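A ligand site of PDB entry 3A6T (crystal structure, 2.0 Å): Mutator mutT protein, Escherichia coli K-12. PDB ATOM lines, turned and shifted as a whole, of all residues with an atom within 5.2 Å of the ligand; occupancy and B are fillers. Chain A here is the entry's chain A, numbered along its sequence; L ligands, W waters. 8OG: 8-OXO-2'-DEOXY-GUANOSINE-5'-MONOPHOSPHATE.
Ile 6 touches the ligand (CG1 to O4', 3.7 Å). CG1 of Val 8 touches N1 of the ligand (3.5 Å). Gly 37 touches the ligand. Gly 38 touches the ligand. CZ of Phe 75 touches O8 of the ligand, 3.4 Å away. CD1 of Ile 80 touches O4' of the ligand (3.5 Å). Leu 82 touches the ligand (CD1 to O8, 3.6 Å). Pro 116 touches the ligand (CB to O8, 3.4 Å). Ala 118 touches the ligand (CB to O8, 3.8 Å). Hydrophobic or aromatic side chains that line the ligand: Ile 6, Val 8, His 28, Phe 35, Phe 75, Ile 80, Leu 82, Pro 116 and Ala 118. 14 residues have an atom within 4 Å of the ligand: Ile 6, Val 8, Arg 23, His 28, Glu 34, Phe 35, Gly 37, Gly 38, Phe 75, Ile 80, Leu 82, Pro 116, Ala 118 and Asn 119. The nearest printed residue that does not touch the ligand is Pro 36 (4.2 Å).
O of His 28 sits at hydrogen-bond distance from NE of Arg 23 (2.8 Å). The guanidinium group of Arg 23 is in salt-bridge range of the side-chain carboxylate of Glu 34 (2.8 Å). The guanidinium group (NE) of Arg 23 sits close to the backbone carbonyl oxygen (O) of Met 29 (3.4 Å). N of Gly 37 is in hydrogen-bond range of OE2 of Glu 57 (3.1 Å).
Water W1 bridges OP2 of the ligand (2.5 Å) and N of Lys 39 (2.9 Å). Water W2 lies within hydrogen-bond range of an oxygen (O3') of the ligand (2.7 Å) and the guanidinium group of Arg 78 (2.7 Å). Water W4 lies within hydrogen-bond range of O of Gly 37 (2.7 Å), OP2 of the ligand (2.8 Å) and NH1 of Arg 23 (3.4 Å).
The side-chain amide oxygen (OD1) of Asn 119 is in hydrogen-bond range of a nitrogen (N7) of the ligand, 2.8 Å away. The guanidinium group (NH2) of Arg 23 is in salt-bridge range of an oxygen (OP1) of the ligand. An oxygen (O3') of the ligand is in hydrogen-bond range of a ring nitrogen (ND1) of His 28, 2.7 Å away. A nitrogen (N2) of the ligand lies within hydrogen-bond range of the side-chain carboxylate (OE2) of Glu 34 (3.0 Å). An oxygen (O6) of the ligand sits at hydrogen-bond distance from the backbone NH of Phe 35, at 3.1 Å. The backbone carbonyl oxygen of Phe 35 lies within hydrogen-bond range of a nitrogen (N1) of the ligand, 2.7 Å away.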
ATOM      1  N   LEU A   4     -27.148 -29.878 -28.036  1.00  0.00           N
ATOM      2  CA  LEU A   4     -26.378 -29.950 -26.802  1.00  0.00           C
ATOM      3  C   LEU A   4     -26.297 -28.595 -26.121  1.00  0.00           C
ATOM      4  O   LEU A   4     -26.256 -27.562 -26.775  1.00  0.00           O
ATOM      5  CB  LEU A   4     -24.949 -30.430 -27.096  1.00  0.00           C
ATOM      6  CG  LEU A   4     -24.719 -31.829 -27.673  1.00  0.00           C
ATOM      7  CD1 LEU A   4     -23.258 -31.960 -28.080  1.00  0.00           C
ATOM      8  CD2 LEU A   4     -25.076 -32.890 -26.636  1.00  0.00           C
ATOM      9  N   ILE A   6     -23.886 -26.580 -23.728  1.00  0.00           N
ATOM     10  CA  ILE A   6     -22.508 -26.614 -23.254  1.00  0.00           C
ATOM     11  C   ILE A   6     -22.148 -25.396 -22.395  1.00  0.00           C
ATOM     12  O   ILE A   6     -22.434 -24.264 -22.768  1.00  0.00           O
ATOM     13  CB  ILE A   6     -21.530 -26.670 -24.454  1.00  0.00           C
ATOM     14  CG1 ILE A   6     -21.878 -27.846 -25.374  1.00  0.00           C
ATOM     15  CG2 ILE A   6     -20.095 -26.771 -23.956  1.00  0.00           C
ATOM     16  CD1 ILE A   6     -21.786 -29.205 -24.708  1.00  0.00           C
ATOM     17  N   VAL A   8     -19.026 -23.327 -20.584  1.00  0.00           N
ATOM     18  CA  VAL A   8     -17.577 -23.162 -20.617  1.00  0.00           C
ATOM     19  C   VAL A   8     -17.163 -21.943 -19.804  1.00  0.00           C
ATOM     20  O   VAL A   8     -17.940 -21.003 -19.609  1.00  0.00           O
ATOM     21  CB  VAL A   8     -17.071 -22.999 -22.079  1.00  0.00           C
ATOM     22  CG1 VAL A   8     -17.665 -24.104 -22.939  1.00  0.00           C
ATOM     23  CG2 VAL A   8     -17.455 -21.635 -22.631  1.00  0.00           C
ATOM     24  N   ARG A  23      -8.211 -29.074 -27.691  1.00  0.00           N
ATOM     25  CA  ARG A  23      -9.005 -30.287 -27.835  1.00  0.00           C
ATOM     26  C   ARG A  23      -8.223 -31.389 -28.542  1.00  0.00           C
ATOM     27  O   ARG A  23      -7.372 -31.116 -29.384  1.00  0.00           O
ATOM     28  CB  ARG A  23     -10.292 -29.977 -28.605  1.00  0.00           C
ATOM     29  CG  ARG A  23     -11.156 -28.932 -27.907  1.00  0.00           C
ATOM     30  CD  ARG A  23     -12.370 -28.580 -28.742  1.00  0.00           C
ATOM     31  NE  ARG A  23     -13.217 -29.738 -29.004  1.00  0.00           N
ATOM     32  CZ  ARG A  23     -14.066 -30.258 -28.118  1.00  0.00           C
ATOM     33  NH1 ARG A  23     -14.185 -29.740 -26.903  1.00  0.00           N
ATOM     34  NH2 ARG A  23     -14.788 -31.317 -28.460  1.00  0.00           N
ATOM     35  N   HIS A  28     -14.597 -33.805 -31.588  1.00  0.00           N
ATOM     36  CA  HIS A  28     -15.306 -32.886 -32.465  1.00  0.00           C
ATOM     37  C   HIS A  28     -14.488 -31.604 -32.325  1.00  0.00           C
ATOM     38  O   HIS A  28     -13.990 -31.319 -31.235  1.00  0.00           O
ATOM     39  CB  HIS A  28     -16.749 -32.684 -31.971  1.00  0.00           C
ATOM     40  CG  HIS A  28     -17.534 -31.713 -32.795  1.00  0.00           C
ATOM     41  ND1 HIS A  28     -17.860 -30.445 -32.356  1.00  0.00           N
ATOM     42  CD2 HIS A  28     -18.060 -31.816 -34.037  1.00  0.00           C
ATOM     43  CE1 HIS A  28     -18.535 -29.809 -33.296  1.00  0.00           C
ATOM     44  NE2 HIS A  28     -18.676 -30.623 -34.329  1.00  0.00           N
ATOM     45  N   MET A  29     -14.336 -30.842 -33.400  1.00  0.00           N
ATOM     46  CA  MET A  29     -13.524 -29.622 -33.355  1.00  0.00           C
ATOM     47  C   MET A  29     -12.119 -30.006 -32.865  1.00  0.00           C
ATOM     48  O   MET A  29     -11.539 -29.357 -31.992  1.00  0.00           O
ATOM     49  CB  MET A  29     -14.150 -28.585 -32.419  1.00  0.00           C
ATOM     50  CG  MET A  29     -15.363 -27.860 -33.007  1.00  0.00           C
ATOM     51  SD  MET A  29     -14.920 -26.886 -34.482  1.00  0.00           S
ATOM     52  CE  MET A  29     -15.629 -27.896 -35.797  1.00  0.00           C
ATOM     53  N   GLU A  34      -9.742 -23.925 -26.898  1.00  0.00           N
ATOM     54  CA  GLU A  34     -11.073 -23.808 -26.337  1.00  0.00           C
ATOM     55  C   GLU A  34     -11.052 -23.285 -24.912  1.00  0.00           C
ATOM     56  O   GLU A  34      -9.996 -23.238 -24.271  1.00  0.00           O
ATOM     57  CB  GLU A  34     -11.753 -25.177 -26.325  1.00  0.00           C
ATOM     58  CG  GLU A  34     -11.011 -26.179 -25.420  1.00  0.00           C
ATOM     59  CD  GLU A  34     -11.861 -27.377 -25.004  1.00  0.00           C
ATOM     60  OE1 GLU A  34     -11.452 -28.073 -24.053  1.00  0.00           O
ATOM     61  OE2 GLU A  34     -12.917 -27.638 -25.615  1.00  0.00           O
ATOM     62  N   PHE A  35     -12.222 -22.878 -24.431  1.00  0.00           N
ATOM     63  CA  PHE A  35     -12.369 -22.451 -23.052  1.00  0.00           C
ATOM     64  C   PHE A  35     -12.758 -23.760 -22.385  1.00  0.00           C
ATOM     65  O   PHE A  35     -13.595 -24.513 -22.905  1.00  0.00           O
ATOM     66  CB  PHE A  35     -13.518 -21.446 -22.914  1.00  0.00           C
ATOM     67  CG  PHE A  35     -13.324 -20.176 -23.681  1.00  0.00           C
ATOM     68  CD1 PHE A  35     -12.222 -19.358 -23.438  1.00  0.00           C
ATOM     69  CD2 PHE A  35     -14.257 -19.782 -24.643  1.00  0.00           C
ATOM     70  CE1 PHE A  35     -12.057 -18.169 -24.142  1.00  0.00           C
ATOM     71  CE2 PHE A  35     -14.094 -18.603 -25.349  1.00  0.00           C
ATOM     72  CZ  PHE A  35     -12.992 -17.787 -25.096  1.00  0.00           C
ATOM     73  N   PRO A  36     -12.152 -24.088 -21.229  1.00  0.00           N
ATOM     74  CA  PRO A  36     -12.540 -25.356 -20.605  1.00  0.00           C
ATOM     75  C   PRO A  36     -14.053 -25.408 -20.372  1.00  0.00           C
ATOM     76  O   PRO A  36     -14.653 -24.426 -19.977  1.00  0.00           O
ATOM     77  CB  PRO A  36     -11.732 -25.364 -19.314  1.00  0.00           C
ATOM     78  CG  PRO A  36     -10.470 -24.640 -19.729  1.00  0.00           C
ATOM     79  CD  PRO A  36     -11.027 -23.468 -20.510  1.00  0.00           C
ATOM     80  N   GLY A  37     -14.658 -26.569 -20.620  1.00  0.00           N
ATOM     81  CA  GLY A  37     -16.081 -26.700 -20.424  1.00  0.00           C
ATOM     82  C   GLY A  37     -16.607 -28.053 -20.855  1.00  0.00           C
ATOM     83  O   GLY A  37     -15.837 -28.935 -21.223  1.00  0.00           O
ATOM     84  N   GLY A  38     -17.923 -28.211 -20.817  1.00  0.00           N
ATOM     85  CA  GLY A  38     -18.524 -29.465 -21.215  1.00  0.00           C
ATOM     86  C   GLY A  38     -20.039 -29.380 -21.182  1.00  0.00           C
ATOM     87  O   GLY A  38     -20.623 -28.341 -20.876  1.00  0.00           O
ATOM     88  N   LYS A  39     -20.677 -30.515 -21.479  1.00  0.00           N
ATOM     89  CA  LYS A  39     -22.128 -30.611 -21.525  1.00  0.00           C
ATOM     90  C   LYS A  39     -22.831 -30.447 -20.173  1.00  0.00           C
ATOM     91  O   LYS A  39     -22.388 -30.987 -19.157  1.00  0.00           O
ATOM     92  CB  LYS A  39     -22.526 -31.946 -22.144  1.00  0.00           C
ATOM     93  CG  LYS A  39     -24.020 -32.219 -22.198  1.00  0.00           C
ATOM     94  CD  LYS A  39     -24.305 -33.566 -22.848  1.00  0.00           C
ATOM     95  CE  LYS A  39     -25.795 -33.867 -22.877  1.00  0.00           C
ATOM     96  NZ  LYS A  39     -26.358 -33.921 -21.491  1.00  0.00           N
ATOM     97  N   GLU A  57     -11.985 -30.550 -15.528  1.00  0.00           N
ATOM     98  CA  GLU A  57     -10.979 -30.276 -16.548  1.00  0.00           C
ATOM     99  C   GLU A  57      -9.692 -29.563 -16.153  1.00  0.00           C
ATOM    100  O   GLU A  57      -8.619 -29.937 -16.616  1.00  0.00           O
ATOM    101  CB  GLU A  57     -11.631 -29.543 -17.722  1.00  0.00           C
ATOM    102  CG  GLU A  57     -12.634 -30.395 -18.473  1.00  0.00           C
ATOM    103  CD  GLU A  57     -12.823 -29.955 -19.902  1.00  0.00           C
ATOM    104  OE1 GLU A  57     -13.228 -30.798 -20.733  1.00  0.00           O
ATOM    105  OE2 GLU A  57     -12.584 -28.770 -20.209  1.00  0.00           O
ATOM    106  N   PHE A  75     -23.324 -26.556 -36.199  1.00  0.00           N
ATOM    107  CA  PHE A  75     -22.168 -27.195 -36.798  1.00  0.00           C
ATOM    108  C   PHE A  75     -22.722 -28.111 -37.894  1.00  0.00           C
ATOM    109  O   PHE A  75     -23.934 -28.351 -37.943  1.00  0.00           O
ATOM    110  CB  PHE A  75     -21.413 -28.021 -35.754  1.00  0.00           C
ATOM    111  CG  PHE A  75     -20.568 -27.190 -34.829  1.00  0.00           C
ATOM    112  CD1 PHE A  75     -19.344 -26.675 -35.257  1.00  0.00           C
ATOM    113  CD2 PHE A  75     -20.978 -26.942 -33.522  1.00  0.00           C
ATOM    114  CE1 PHE A  75     -18.541 -25.927 -34.394  1.00  0.00           C
ATOM    115  CE2 PHE A  75     -20.176 -26.196 -32.649  1.00  0.00           C
ATOM    116  CZ  PHE A  75     -18.962 -25.687 -33.090  1.00  0.00           C
ATOM    117  N   ARG A  78     -24.333 -31.058 -35.808  1.00  0.00           N
ATOM    118  CA  ARG A  78     -24.916 -30.866 -34.490  1.00  0.00           C
ATOM    119  C   ARG A  78     -25.188 -29.405 -34.172  1.00  0.00           C
ATOM    120  O   ARG A  78     -24.528 -28.504 -34.696  1.00  0.00           O
ATOM    121  CB  ARG A  78     -24.011 -31.477 -33.409  1.00  0.00           C
ATOM    122  CG  ARG A  78     -22.682 -30.770 -33.216  1.00  0.00           C
ATOM    123  CD  ARG A  78     -21.717 -31.674 -32.462  1.00  0.00           C
ATOM    124  NE  ARG A  78     -21.274 -32.784 -33.298  1.00  0.00           N
ATOM    125  CZ  ARG A  78     -20.615 -33.853 -32.844  1.00  0.00           C
ATOM    126  NH1 ARG A  78     -20.334 -33.956 -31.555  1.00  0.00           N
ATOM    127  NH2 ARG A  78     -20.244 -34.804 -33.688  1.00  0.00           N
ATOM    128  N   ILE A  80     -25.477 -26.686 -31.081  1.00  0.00           N
ATOM    129  CA  ILE A  80     -25.123 -26.515 -29.680  1.00  0.00           C
ATOM    130  C   ILE A  80     -25.409 -25.114 -29.170  1.00  0.00           C
ATOM    131  O   ILE A  80     -25.320 -24.124 -29.900  1.00  0.00           O
ATOM    132  CB  ILE A  80     -23.628 -26.824 -29.421  1.00  0.00           C
ATOM    133  CG1 ILE A  80     -22.760 -25.672 -29.927  1.00  0.00           C
ATOM    134  CG2 ILE A  80     -23.229 -28.123 -30.115  1.00  0.00           C
ATOM    135  CD1 ILE A  80     -21.340 -25.756 -29.448  1.00  0.00           C
ATOM    136  N   LEU A  82     -24.086 -22.565 -26.417  1.00  0.00           N
ATOM    137  CA  LEU A  82     -22.918 -22.339 -25.587  1.00  0.00           C
ATOM    138  C   LEU A  82     -23.136 -21.258 -24.549  1.00  0.00           C
ATOM    139  O   LEU A  82     -23.597 -20.170 -24.866  1.00  0.00           O
ATOM    140  CB  LEU A  82     -21.712 -21.976 -26.456  1.00  0.00           C
ATOM    141  CG  LEU A  82     -21.043 -23.114 -27.243  1.00  0.00           C
ATOM    142  CD1 LEU A  82     -20.338 -22.558 -28.475  1.00  0.00           C
ATOM    143  CD2 LEU A  82     -20.046 -23.838 -26.339  1.00  0.00           C
ATOM    144  N   PHE A  84     -21.078 -19.018 -22.199  1.00  0.00           N
ATOM    145  CA  PHE A  84     -19.737 -18.542 -21.906  1.00  0.00           C
ATOM    146  C   PHE A  84     -19.721 -17.755 -20.594  1.00  0.00           C
ATOM    147  O   PHE A  84     -20.223 -16.637 -20.531  1.00  0.00           O
ATOM    148  CB  PHE A  84     -19.241 -17.649 -23.043  1.00  0.00           C
ATOM    149  CG  PHE A  84     -19.079 -18.360 -24.363  1.00  0.00           C
ATOM    150  CD1 PHE A  84     -17.874 -18.970 -24.695  1.00  0.00           C
ATOM    151  CD2 PHE A  84     -20.128 -18.414 -25.270  1.00  0.00           C
ATOM    152  CE1 PHE A  84     -17.707 -19.619 -25.920  1.00  0.00           C
ATOM    153  CE2 PHE A  84     -19.980 -19.059 -26.497  1.00  0.00           C
ATOM    154  CZ  PHE A  84     -18.774 -19.660 -26.827  1.00  0.00           C
ATOM    155  N   PHE A 115      -9.909 -21.220 -32.573  1.00  0.00           N
ATOM    156  CA  PHE A 115     -11.031 -21.773 -31.804  1.00  0.00           C
ATOM    157  C   PHE A 115     -12.184 -22.217 -32.695  1.00  0.00           C
ATOM    158  O   PHE A 115     -12.200 -21.910 -33.887  1.00  0.00           O
ATOM    159  CB  PHE A 115     -11.599 -20.733 -30.830  1.00  0.00           C
ATOM    160  CG  PHE A 115     -10.619 -20.237 -29.803  1.00  0.00           C
ATOM    161  CD1 PHE A 115      -9.543 -19.452 -30.163  1.00  0.00           C
ATOM    162  CD2 PHE A 115     -10.792 -20.575 -28.463  1.00  0.00           C
ATOM    163  CE1 PHE A 115      -8.637 -18.999 -29.213  1.00  0.00           C
ATOM    164  CE2 PHE A 115      -9.900 -20.134 -27.496  1.00  0.00           C
ATOM    165  CZ  PHE A 115      -8.822 -19.345 -27.876  1.00  0.00           C
ATOM    166  N   PRO A 116     -13.161 -22.946 -32.140  1.00  0.00           N
ATOM    167  CA  PRO A 116     -14.293 -23.367 -32.964  1.00  0.00           C
ATOM    168  C   PRO A 116     -14.950 -22.089 -33.479  1.00  0.00           C
ATOM    169  O   PRO A 116     -14.938 -21.053 -32.805  1.00  0.00           O
ATOM    170  CB  PRO A 116     -15.181 -24.118 -31.983  1.00  0.00           C
ATOM    171  CG  PRO A 116     -14.165 -24.737 -31.057  1.00  0.00           C
ATOM    172  CD  PRO A 116     -13.216 -23.583 -30.805  1.00  0.00           C
ATOM    173  N   ALA A 118     -17.872 -21.134 -33.493  1.00  0.00           N
ATOM    174  CA  ALA A 118     -18.933 -20.654 -32.608  1.00  0.00           C
ATOM    175  C   ALA A 118     -18.419 -19.603 -31.623  1.00  0.00           C
ATOM    176  O   ALA A 118     -19.189 -18.789 -31.135  1.00  0.00           O
ATOM    177  CB  ALA A 118     -19.547 -21.821 -31.844  1.00  0.00           C
ATOM    178  N   ASN A 119     -17.117 -19.624 -31.349  1.00  0.00           N
ATOM    179  CA  ASN A 119     -16.487 -18.685 -30.415  1.00  0.00           C
ATOM    180  C   ASN A 119     -16.164 -17.304 -30.983  1.00  0.00           C
ATOM    181  O   ASN A 119     -15.830 -16.379 -30.236  1.00  0.00           O
ATOM    182  CB  ASN A 119     -15.202 -19.309 -29.871  1.00  0.00           C
ATOM    183  CG  ASN A 119     -15.454 -20.533 -29.030  1.00  0.00           C
ATOM    184  OD1 ASN A 119     -16.392 -21.294 -29.285  1.00  0.00           O
ATOM    185  ND2 ASN A 119     -14.606 -20.764 -28.035  1.00  0.00           N
HETATM  186  OP3 8OG L   1     -18.112 -33.358 -25.710  1.00  0.00           O
HETATM  187  P   8OG L   1     -17.582 -31.990 -25.450  1.00  0.00           P
HETATM  188  OP1 8OG L   1     -16.323 -31.854 -26.215  1.00  0.00           O
HETATM  189  OP2 8OG L   1     -17.536 -31.811 -23.987  1.00  0.00           O
HETATM  190  O5' 8OG L   1     -18.668 -30.965 -26.039  1.00  0.00           O
HETATM  191  C5' 8OG L   1     -18.338 -29.592 -26.280  1.00  0.00           C
HETATM  192  C4' 8OG L   1     -18.912 -29.107 -27.617  1.00  0.00           C
HETATM  193  O4' 8OG L   1     -19.001 -27.664 -27.652  1.00  0.00           O
HETATM  194  C3' 8OG L   1     -18.053 -29.528 -28.808  1.00  0.00           C
HETATM  195  O3' 8OG L   1     -18.895 -29.909 -29.901  1.00  0.00           O
HETATM  196  C2' 8OG L   1     -17.237 -28.307 -29.110  1.00  0.00           C
HETATM  197  C1' 8OG L   1     -18.165 -27.167 -28.708  1.00  0.00           C
HETATM  198  N9  8OG L   1     -17.397 -25.985 -28.255  1.00  0.00           N
HETATM  199  C8  8OG L   1     -17.307 -24.814 -28.960  1.00  0.00           C
HETATM  200  N7  8OG L   1     -16.597 -23.911 -28.413  1.00  0.00           N
HETATM  201  C5  8OG L   1     -16.126 -24.461 -27.222  1.00  0.00           C
HETATM  202  C6  8OG L   1     -15.286 -23.943 -26.185  1.00  0.00           C
HETATM  203  O6  8OG L   1     -14.771 -22.834 -26.110  1.00  0.00           O
HETATM  204  N1  8OG L   1     -15.090 -24.881 -25.149  1.00  0.00           N
HETATM  205  C2  8OG L   1     -15.627 -26.176 -25.109  1.00  0.00           C
HETATM  206  N2  8OG L   1     -15.327 -26.920 -24.045  1.00  0.00           N
HETATM  207  N3  8OG L   1     -16.417 -26.674 -26.086  1.00  0.00           N
HETATM  208  C4  8OG L   1     -16.631 -25.777 -27.111  1.00  0.00           C
HETATM  209  O8  8OG L   1     -17.896 -24.702 -30.043  1.00  0.00           O
HETATM  210  O   HOH W   1     -19.075 -32.773 -22.224  1.00  0.00           O
HETATM  211  O   HOH W   2     -20.163 -32.249 -29.434  1.00  0.00           O
HETATM  212  O   HOH W   3     -14.088 -33.314 -25.572  1.00  0.00           O
HETATM  213  O   HOH W   4     -15.600 -29.807 -23.796  1.00  0.00           O
HETATM  214  O   HOH W   5     -18.134 -33.681 -28.366  1.00  0.00           O
